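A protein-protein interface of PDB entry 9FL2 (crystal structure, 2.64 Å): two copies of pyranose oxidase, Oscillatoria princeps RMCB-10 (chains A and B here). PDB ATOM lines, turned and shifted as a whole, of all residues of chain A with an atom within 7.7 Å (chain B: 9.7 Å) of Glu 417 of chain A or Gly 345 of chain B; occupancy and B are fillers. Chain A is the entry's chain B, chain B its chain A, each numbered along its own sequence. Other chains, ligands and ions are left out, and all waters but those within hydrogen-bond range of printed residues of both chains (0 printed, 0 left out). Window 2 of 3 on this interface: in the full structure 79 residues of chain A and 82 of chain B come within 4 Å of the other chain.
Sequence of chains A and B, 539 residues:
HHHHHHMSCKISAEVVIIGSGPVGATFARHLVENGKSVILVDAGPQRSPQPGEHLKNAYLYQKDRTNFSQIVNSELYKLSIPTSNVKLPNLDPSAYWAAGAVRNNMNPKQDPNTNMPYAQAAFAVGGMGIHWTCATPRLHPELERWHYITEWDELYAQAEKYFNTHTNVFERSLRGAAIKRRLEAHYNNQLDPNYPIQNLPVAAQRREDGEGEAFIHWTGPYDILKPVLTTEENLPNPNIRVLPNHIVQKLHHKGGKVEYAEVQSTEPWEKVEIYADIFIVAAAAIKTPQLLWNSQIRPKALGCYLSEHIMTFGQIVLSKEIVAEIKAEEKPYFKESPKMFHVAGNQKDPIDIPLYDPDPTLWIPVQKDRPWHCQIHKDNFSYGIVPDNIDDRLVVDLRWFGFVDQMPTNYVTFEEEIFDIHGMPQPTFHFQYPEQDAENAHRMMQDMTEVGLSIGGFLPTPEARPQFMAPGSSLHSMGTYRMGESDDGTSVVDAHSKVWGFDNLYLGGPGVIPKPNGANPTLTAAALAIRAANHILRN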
ATOM      1  N   VAL A 102     -18.604  13.139 -12.523  1.00  0.00           N
ATOM      2  CA  VAL A 102     -19.607  13.437 -11.514  1.00  0.00           C
ATOM      3  C   VAL A 102     -20.815  14.114 -12.145  1.00  0.00           C
ATOM      4  O   VAL A 102     -21.765  14.507 -11.469  1.00  0.00           O
ATOM      5  CB  VAL A 102     -18.975  14.359 -10.461  1.00  0.00           C
ATOM      6  CG1 VAL A 102     -17.979  13.619  -9.581  1.00  0.00           C
ATOM      7  CG2 VAL A 102     -18.333  15.579 -11.113  1.00  0.00           C
ATOM      8  N   LYS A 109     -18.843   7.467  -6.230  1.00  0.00           N
ATOM      9  CA  LYS A 109     -18.911   6.836  -4.920  1.00  0.00           C
ATOM     10  C   LYS A 109     -19.779   5.593  -5.000  1.00  0.00           C
ATOM     11  O   LYS A 109     -19.905   4.920  -3.989  1.00  0.00           O
ATOM     12  CB  LYS A 109     -19.517   7.732  -3.829  1.00  0.00           C
ATOM     13  CG  LYS A 109     -18.833   9.080  -3.606  1.00  0.00           C
ATOM     14  CD  LYS A 109     -18.114   9.313  -2.283  1.00  0.00           C
ATOM     15  CE  LYS A 109     -18.219  10.761  -1.913  1.00  0.00           C
ATOM     16  NZ  LYS A 109     -17.270  11.074  -0.854  1.00  0.00           N
ATOM     17  N   PHE A 414     -27.604   9.504   0.148  1.00  0.00           N
ATOM     18  CA  PHE A 414     -27.462  10.708  -0.657  1.00  0.00           C
ATOM     19  C   PHE A 414     -26.163  11.426  -0.292  1.00  0.00           C
ATOM     20  O   PHE A 414     -25.994  11.845   0.856  1.00  0.00           O
ATOM     21  CB  PHE A 414     -28.718  11.557  -0.444  1.00  0.00           C
ATOM     22  CG  PHE A 414     -30.020  10.941  -0.951  1.00  0.00           C
ATOM     23  CD1 PHE A 414     -30.368  11.000  -2.297  1.00  0.00           C
ATOM     24  CD2 PHE A 414     -30.903  10.325  -0.071  1.00  0.00           C
ATOM     25  CE1 PHE A 414     -31.555  10.447  -2.739  1.00  0.00           C
ATOM     26  CE2 PHE A 414     -32.086   9.767  -0.529  1.00  0.00           C
ATOM     27  CZ  PHE A 414     -32.412   9.831  -1.856  1.00  0.00           C
ATOM     28  N   GLU A 415     -25.272  11.589  -1.283  1.00  0.00           N
ATOM     29  CA  GLU A 415     -23.972  12.181  -1.032  1.00  0.00           C
ATOM     30  C   GLU A 415     -24.180  13.649  -0.673  1.00  0.00           C
ATOM     31  O   GLU A 415     -25.146  14.263  -1.134  1.00  0.00           O
ATOM     32  CB  GLU A 415     -23.061  12.044  -2.247  1.00  0.00           C
ATOM     33  CG  GLU A 415     -22.822  10.626  -2.741  1.00  0.00           C
ATOM     34  CD  GLU A 415     -22.355   9.591  -1.737  1.00  0.00           C
ATOM     35  OE1 GLU A 415     -22.568   9.798  -0.529  1.00  0.00           O
ATOM     36  OE2 GLU A 415     -21.840   8.552  -2.176  1.00  0.00           O
ATOM     37  N   GLU A 416     -23.285  14.186   0.163  1.00  0.00           N
ATOM     38  CA  GLU A 416     -23.354  15.584   0.550  1.00  0.00           C
ATOM     39  C   GLU A 416     -22.571  16.464  -0.421  1.00  0.00           C
ATOM     40  O   GLU A 416     -22.884  17.645  -0.558  1.00  0.00           O
ATOM     41  CB  GLU A 416     -22.829  15.767   1.974  1.00  0.00           C
ATOM     42  CG  GLU A 416     -23.376  14.737   2.957  1.00  0.00           C
ATOM     43  CD  GLU A 416     -22.376  13.828   3.643  1.00  0.00           C
ATOM     44  OE1 GLU A 416     -21.172  14.146   3.660  1.00  0.00           O
ATOM     45  OE2 GLU A 416     -22.831  12.801   4.189  1.00  0.00           O
ATOM     46  N   GLU A 417     -21.578  15.888  -1.122  1.00  0.00           N
ATOM     47  CA  GLU A 417     -20.667  16.649  -1.970  1.00  0.00           C
ATOM     48  C   GLU A 417     -20.806  16.288  -3.455  1.00  0.00           C
ATOM     49  O   GLU A 417     -19.944  16.656  -4.253  1.00  0.00           O
ATOM     50  CB  GLU A 417     -19.229  16.389  -1.522  1.00  0.00           C
ATOM     51  CG  GLU A 417     -18.930  16.950  -0.136  1.00  0.00           C
ATOM     52  CD  GLU A 417     -17.504  16.706   0.327  1.00  0.00           C
ATOM     53  OE1 GLU A 417     -17.038  15.555   0.168  1.00  0.00           O
ATOM     54  OE2 GLU A 417     -16.868  17.650   0.847  1.00  0.00           O
ATOM     55  N   ILE A 418     -21.864  15.557  -3.832  1.00  0.00           N
ATOM     56  CA  ILE A 418     -22.100  15.237  -5.227  1.00  0.00           C
ATOM     57  C   ILE A 418     -23.572  15.510  -5.510  1.00  0.00           C
ATOM     58  O   ILE A 418     -24.395  15.382  -4.615  1.00  0.00           O
ATOM     59  CB  ILE A 418     -21.676  13.790  -5.550  1.00  0.00           C
ATOM     60  CG1 ILE A 418     -20.255  13.508  -5.033  1.00  0.00           C
ATOM     61  CG2 ILE A 418     -21.840  13.481  -7.050  1.00  0.00           C
ATOM     62  CD1 ILE A 418     -19.701  12.138  -5.375  1.00  0.00           C
ATOM     63  N   PHE A 419     -23.891  15.916  -6.745  1.00  0.00           N
ATOM     64  CA  PHE A 419     -25.261  16.245  -7.095  1.00  0.00           C
ATOM     65  C   PHE A 419     -25.592  15.622  -8.451  1.00  0.00           C
ATOM     66  O   PHE A 419     -24.719  15.216  -9.234  1.00  0.00           O
ATOM     67  CB  PHE A 419     -25.486  17.761  -7.004  1.00  0.00           C
ATOM     68  CG  PHE A 419     -25.035  18.385  -5.683  1.00  0.00           C
ATOM     69  CD1 PHE A 419     -23.713  18.780  -5.485  1.00  0.00           C
ATOM     70  CD2 PHE A 419     -25.919  18.558  -4.622  1.00  0.00           C
ATOM     71  CE1 PHE A 419     -23.294  19.327  -4.275  1.00  0.00           C
ATOM     72  CE2 PHE A 419     -25.495  19.103  -3.410  1.00  0.00           C
ATOM     73  CZ  PHE A 419     -24.185  19.480  -3.239  1.00  0.00           C
ATOM     74  N   PRO A 425     -28.812  16.178  -4.029  1.00  0.00           N
ATOM     75  CA  PRO A 425     -27.891  15.150  -3.549  1.00  0.00           C
ATOM     76  C   PRO A 425     -27.892  13.882  -4.400  1.00  0.00           C
ATOM     77  O   PRO A 425     -28.935  13.280  -4.639  1.00  0.00           O
ATOM     78  CB  PRO A 425     -28.416  14.930  -2.139  1.00  0.00           C
ATOM     79  CG  PRO A 425     -28.831  16.318  -1.708  1.00  0.00           C
ATOM     80  CD  PRO A 425     -29.531  16.854  -2.932  1.00  0.00           C
ATOM     81  N   GLN A 426     -26.703  13.523  -4.885  1.00  0.00           N
ATOM     82  CA  GLN A 426     -26.532  12.348  -5.723  1.00  0.00           C
ATOM     83  C   GLN A 426     -26.928  11.116  -4.918  1.00  0.00           C
ATOM     84  O   GLN A 426     -26.397  10.891  -3.832  1.00  0.00           O
ATOM     85  CB  GLN A 426     -25.072  12.196  -6.152  1.00  0.00           C
ATOM     86  CG  GLN A 426     -24.759  10.917  -6.929  1.00  0.00           C
ATOM     87  CD  GLN A 426     -25.500  10.839  -8.243  1.00  0.00           C
ATOM     88  OE1 GLN A 426     -25.313  11.685  -9.139  1.00  0.00           O
ATOM     89  NE2 GLN A 426     -26.335   9.811  -8.363  1.00  0.00           N
ATOM     90  N   PRO B 338     -23.802  27.148  -7.464  1.00  0.00           N
ATOM     91  CA  PRO B 338     -22.688  26.196  -7.417  1.00  0.00           C
ATOM     92  C   PRO B 338     -23.050  24.733  -7.650  1.00  0.00           C
ATOM     93  O   PRO B 338     -22.223  23.992  -8.177  1.00  0.00           O
ATOM     94  CB  PRO B 338     -22.073  26.410  -6.013  1.00  0.00           C
ATOM     95  CG  PRO B 338     -22.392  27.846  -5.689  1.00  0.00           C
ATOM     96  CD  PRO B 338     -23.753  28.109  -6.348  1.00  0.00           C
ATOM     97  N   LYS B 339     -24.267  24.320  -7.261  1.00  0.00           N
ATOM     98  CA  LYS B 339     -24.656  22.914  -7.271  1.00  0.00           C
ATOM     99  C   LYS B 339     -24.916  22.426  -8.698  1.00  0.00           C
ATOM    100  O   LYS B 339     -25.207  21.251  -8.913  1.00  0.00           O
ATOM    101  CB  LYS B 339     -25.892  22.657  -6.391  1.00  0.00           C
ATOM    102  CG  LYS B 339     -25.670  22.654  -4.895  1.00  0.00           C
ATOM    103  CD  LYS B 339     -26.940  22.788  -4.069  1.00  0.00           C
ATOM    104  CE  LYS B 339     -26.605  22.969  -2.624  1.00  0.00           C
ATOM    105  NZ  LYS B 339     -27.861  23.082  -1.887  1.00  0.00           N
ATOM    106  N   PHE B 341     -22.676  22.457 -10.938  1.00  0.00           N
ATOM    107  CA  PHE B 341     -21.418  21.831 -11.330  1.00  0.00           C
ATOM    108  C   PHE B 341     -21.241  20.469 -10.656  1.00  0.00           C
ATOM    109  O   PHE B 341     -20.229  19.818 -10.886  1.00  0.00           O
ATOM    110  CB  PHE B 341     -20.254  22.744 -10.939  1.00  0.00           C
ATOM    111  CG  PHE B 341     -20.231  24.075 -11.678  1.00  0.00           C
ATOM    112  CD1 PHE B 341     -20.995  25.149 -11.237  1.00  0.00           C
ATOM    113  CD2 PHE B 341     -19.432  24.246 -12.809  1.00  0.00           C
ATOM    114  CE1 PHE B 341     -20.933  26.365 -11.907  1.00  0.00           C
ATOM    115  CE2 PHE B 341     -19.380  25.464 -13.469  1.00  0.00           C
ATOM    116  CZ  PHE B 341     -20.143  26.517 -13.026  1.00  0.00           C
ATOM    117  N   HIS B 342     -22.211  20.070  -9.822  1.00  0.00           N
ATOM    118  CA  HIS B 342     -22.306  18.744  -9.221  1.00  0.00           C
ATOM    119  C   HIS B 342     -21.185  18.442  -8.215  1.00  0.00           C
ATOM    120  O   HIS B 342     -20.958  17.258  -7.934  1.00  0.00           O
ATOM    121  CB  HIS B 342     -22.316  17.614 -10.263  1.00  0.00           C
ATOM    122  CG  HIS B 342     -23.215  17.846 -11.414  1.00  0.00           C
ATOM    123  ND1 HIS B 342     -24.580  17.962 -11.287  1.00  0.00           N
ATOM    124  CD2 HIS B 342     -22.926  18.031 -12.713  1.00  0.00           C
ATOM    125  CE1 HIS B 342     -25.098  18.218 -12.486  1.00  0.00           C
ATOM    126  NE2 HIS B 342     -24.108  18.259 -13.370  1.00  0.00           N
ATOM    127  N   VAL B 343     -20.514  19.466  -7.654  1.00  0.00           N
ATOM    128  CA  VAL B 343     -19.513  19.203  -6.622  1.00  0.00           C
ATOM    129  C   VAL B 343     -19.511  20.322  -5.580  1.00  0.00           C
ATOM    130  O   VAL B 343     -19.860  21.465  -5.865  1.00  0.00           O
ATOM    131  CB  VAL B 343     -18.084  18.944  -7.148  1.00  0.00           C
ATOM    132  CG1 VAL B 343     -17.950  17.593  -7.841  1.00  0.00           C
ATOM    133  CG2 VAL B 343     -17.561  20.064  -8.034  1.00  0.00           C
ATOM    134  N   ALA B 344     -19.117  19.946  -4.359  1.00  0.00           N
ATOM    135  CA  ALA B 344     -18.984  20.871  -3.250  1.00  0.00           C
ATOM    136  C   ALA B 344     -18.009  20.295  -2.224  1.00  0.00           C
ATOM    137  O   ALA B 344     -17.792  19.082  -2.177  1.00  0.00           O
ATOM    138  CB  ALA B 344     -20.343  21.134  -2.641  1.00  0.00           C
ATOM    139  N   GLY B 345     -17.407  21.188  -1.425  1.00  0.00           N
ATOM    140  CA  GLY B 345     -16.381  20.824  -0.466  1.00  0.00           C
ATOM    141  C   GLY B 345     -15.233  20.063  -1.129  1.00  0.00           C
ATOM    142  O   GLY B 345     -14.650  20.520  -2.114  1.00  0.00           O
ATOM    143  N   ASN B 346     -14.957  18.869  -0.586  1.00  0.00           N
ATOM    144  CA  ASN B 346     -13.748  18.117  -0.874  1.00  0.00           C
ATOM    145  C   ASN B 346     -13.774  17.482  -2.266  1.00  0.00           C
ATOM    146  O   ASN B 346     -12.723  17.130  -2.785  1.00  0.00           O
ATOM    147  CB  ASN B 346     -13.543  17.033   0.180  1.00  0.00           C
ATOM    148  CG  ASN B 346     -12.121  17.017   0.668  1.00  0.00           C
ATOM    149  OD1 ASN B 346     -11.623  18.068   1.086  1.00  0.00           O
ATOM    150  ND2 ASN B 346     -11.460  15.872   0.590  1.00  0.00           N
ATOM    151  N   GLN B 347     -14.968  17.266  -2.818  1.00  0.00           N
ATOM    152  CA  GLN B 347     -15.089  16.643  -4.119  1.00  0.00           C
ATOM    153  C   GLN B 347     -14.845  17.702  -5.189  1.00  0.00           C
ATOM    154  O   GLN B 347     -15.398  18.801  -5.102  1.00  0.00           O
ATOM    155  CB  GLN B 347     -16.479  16.034  -4.283  1.00  0.00           C
ATOM    156  CG  GLN B 347     -16.623  15.146  -5.512  1.00  0.00           C
ATOM    157  CD  GLN B 347     -15.986  13.787  -5.331  1.00  0.00           C
ATOM    158  OE1 GLN B 347     -16.146  13.141  -4.284  1.00  0.00           O
ATOM    159  NE2 GLN B 347     -15.278  13.330  -6.357  1.00  0.00           N
ATOM    160  N   LYS B 348     -14.006  17.364  -6.174  1.00  0.00           N
ATOM    161  CA  LYS B 348     -13.848  18.179  -7.373  1.00  0.00           C
ATOM    162  C   LYS B 348     -14.216  17.351  -8.603  1.00  0.00           C
ATOM    163  O   LYS B 348     -14.298  16.130  -8.553  1.00  0.00           O
ATOM    164  CB  LYS B 348     -12.433  18.773  -7.508  1.00  0.00           C
ATOM    165  CG  LYS B 348     -12.111  20.065  -6.702  1.00  0.00           C
ATOM    166  CD  LYS B 348     -12.178  19.987  -5.167  1.00  0.00           C
ATOM    167  CE  LYS B 348     -11.260  20.897  -4.406  1.00  0.00           C
ATOM    168  NZ  LYS B 348     -11.620  22.304  -4.585  1.00  0.00           N
ATOM    169  N   ASP B 349     -14.440  18.040  -9.717  1.00  0.00           N
ATOM    170  CA  ASP B 349     -14.737  17.379 -10.974  1.00  0.00           C
ATOM    171  C   ASP B 349     -13.419  17.024 -11.652  1.00  0.00           C
ATOM    172  O   ASP B 349     -12.690  17.920 -12.050  1.00  0.00           O
ATOM    173  CB  ASP B 349     -15.562  18.290 -11.865  1.00  0.00           C
ATOM    174  CG  ASP B 349     -15.919  17.710 -13.219  1.00  0.00           C
ATOM    175  OD1 ASP B 349     -15.812  16.488 -13.413  1.00  0.00           O
ATOM    176  OD2 ASP B 349     -16.264  18.495 -14.087  1.00  0.00           O
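Hydrophobic or aromatic side chains of chain A within 4 Å of the printed part of chain B: Val 102, Ile 418 and Phe 419. Hydrophobic or aromatic side chains of chain B within 4 Å of the printed part of chain A: His 342, Val 343 and Ala 344. Among the printed residues, 16 pairs touch across the chains.
The backbone carbonyl oxygen of Ile 418 of chain A lies within hydrogen-bond range of the backbone NH of Gln 426 of chain A (3.0 Å).
A ring nitrogen (ND1) of His 342 of chain B sits at hydrogen-bond distance from the backbone carbonyl oxygen of Phe 419 of chain A. The backbone carbonyl oxygen (O) of Glu 417 of chain A is in hydrogen-bond range of the backbone NH (N) of Ala 344 of chain B. The side-chain carboxylate (OE2) of Glu 417 of chain A is in hydrogen-bond range of the backbone NH (N) of Asn 346 of chain B, at 2.7 Å.
No position is printed for both chains.
Of chain B, only His 342 (3.9 Å), Val 343 (3.5 Å), Ala 344 (3.1 Å), Gly 345 (3.5 Å), Asn 346 (2.7 Å) and Gln 347 (3.5 Å) come within 4 Å of Glu 417 of chain A. Ala 344 of chain B touches just these residues of chain A: Glu 417 and Phe 419. Gly 345 of chain B touches just one residue of chain A: Glu 417 (3.5 Å). Printed residues of chain A within 4 Å of Gln 347 of chain B: Lys 109, Glu 417 and Ile 418. Of the printed residues of chain A, Asp 349 of chain B touches Val 102 (3.5 Å). The nearest printed residue of chain A that does not touch Val 343 of chain B is Ile 418 of chain A (4.9 Å).
O of Val 102 of chain A touches CB of His 342 of chain B (3.4 Å). Val 343 of chain B touches Val 102 of chain A. Val 102 of chain A touches Asp 349 of chain B (CG2 to OD1, 3.5 Å). His 342 of chain B touches Glu 417 of chain A (O to O, 3.9 Å). Glu 417 of chain A touches Val 343 of chain B (O to CA, 3.5 Å). OE2 of Glu 417 of chain A touches CA of Gly 345 of chain B (3.5 Å). Glu 417 of chain A touches Gln 347 of chain B (O to CB, 3.5 Å). O of His 342 of chain B touches CA of Ile 418 of chain A (3.6 Å). CD1 of Ile 418 of chain A touches OE1 of Gln 347 of chain B (3.9 Å). Phe 419 of chain A touches Lys 339 of chain B.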
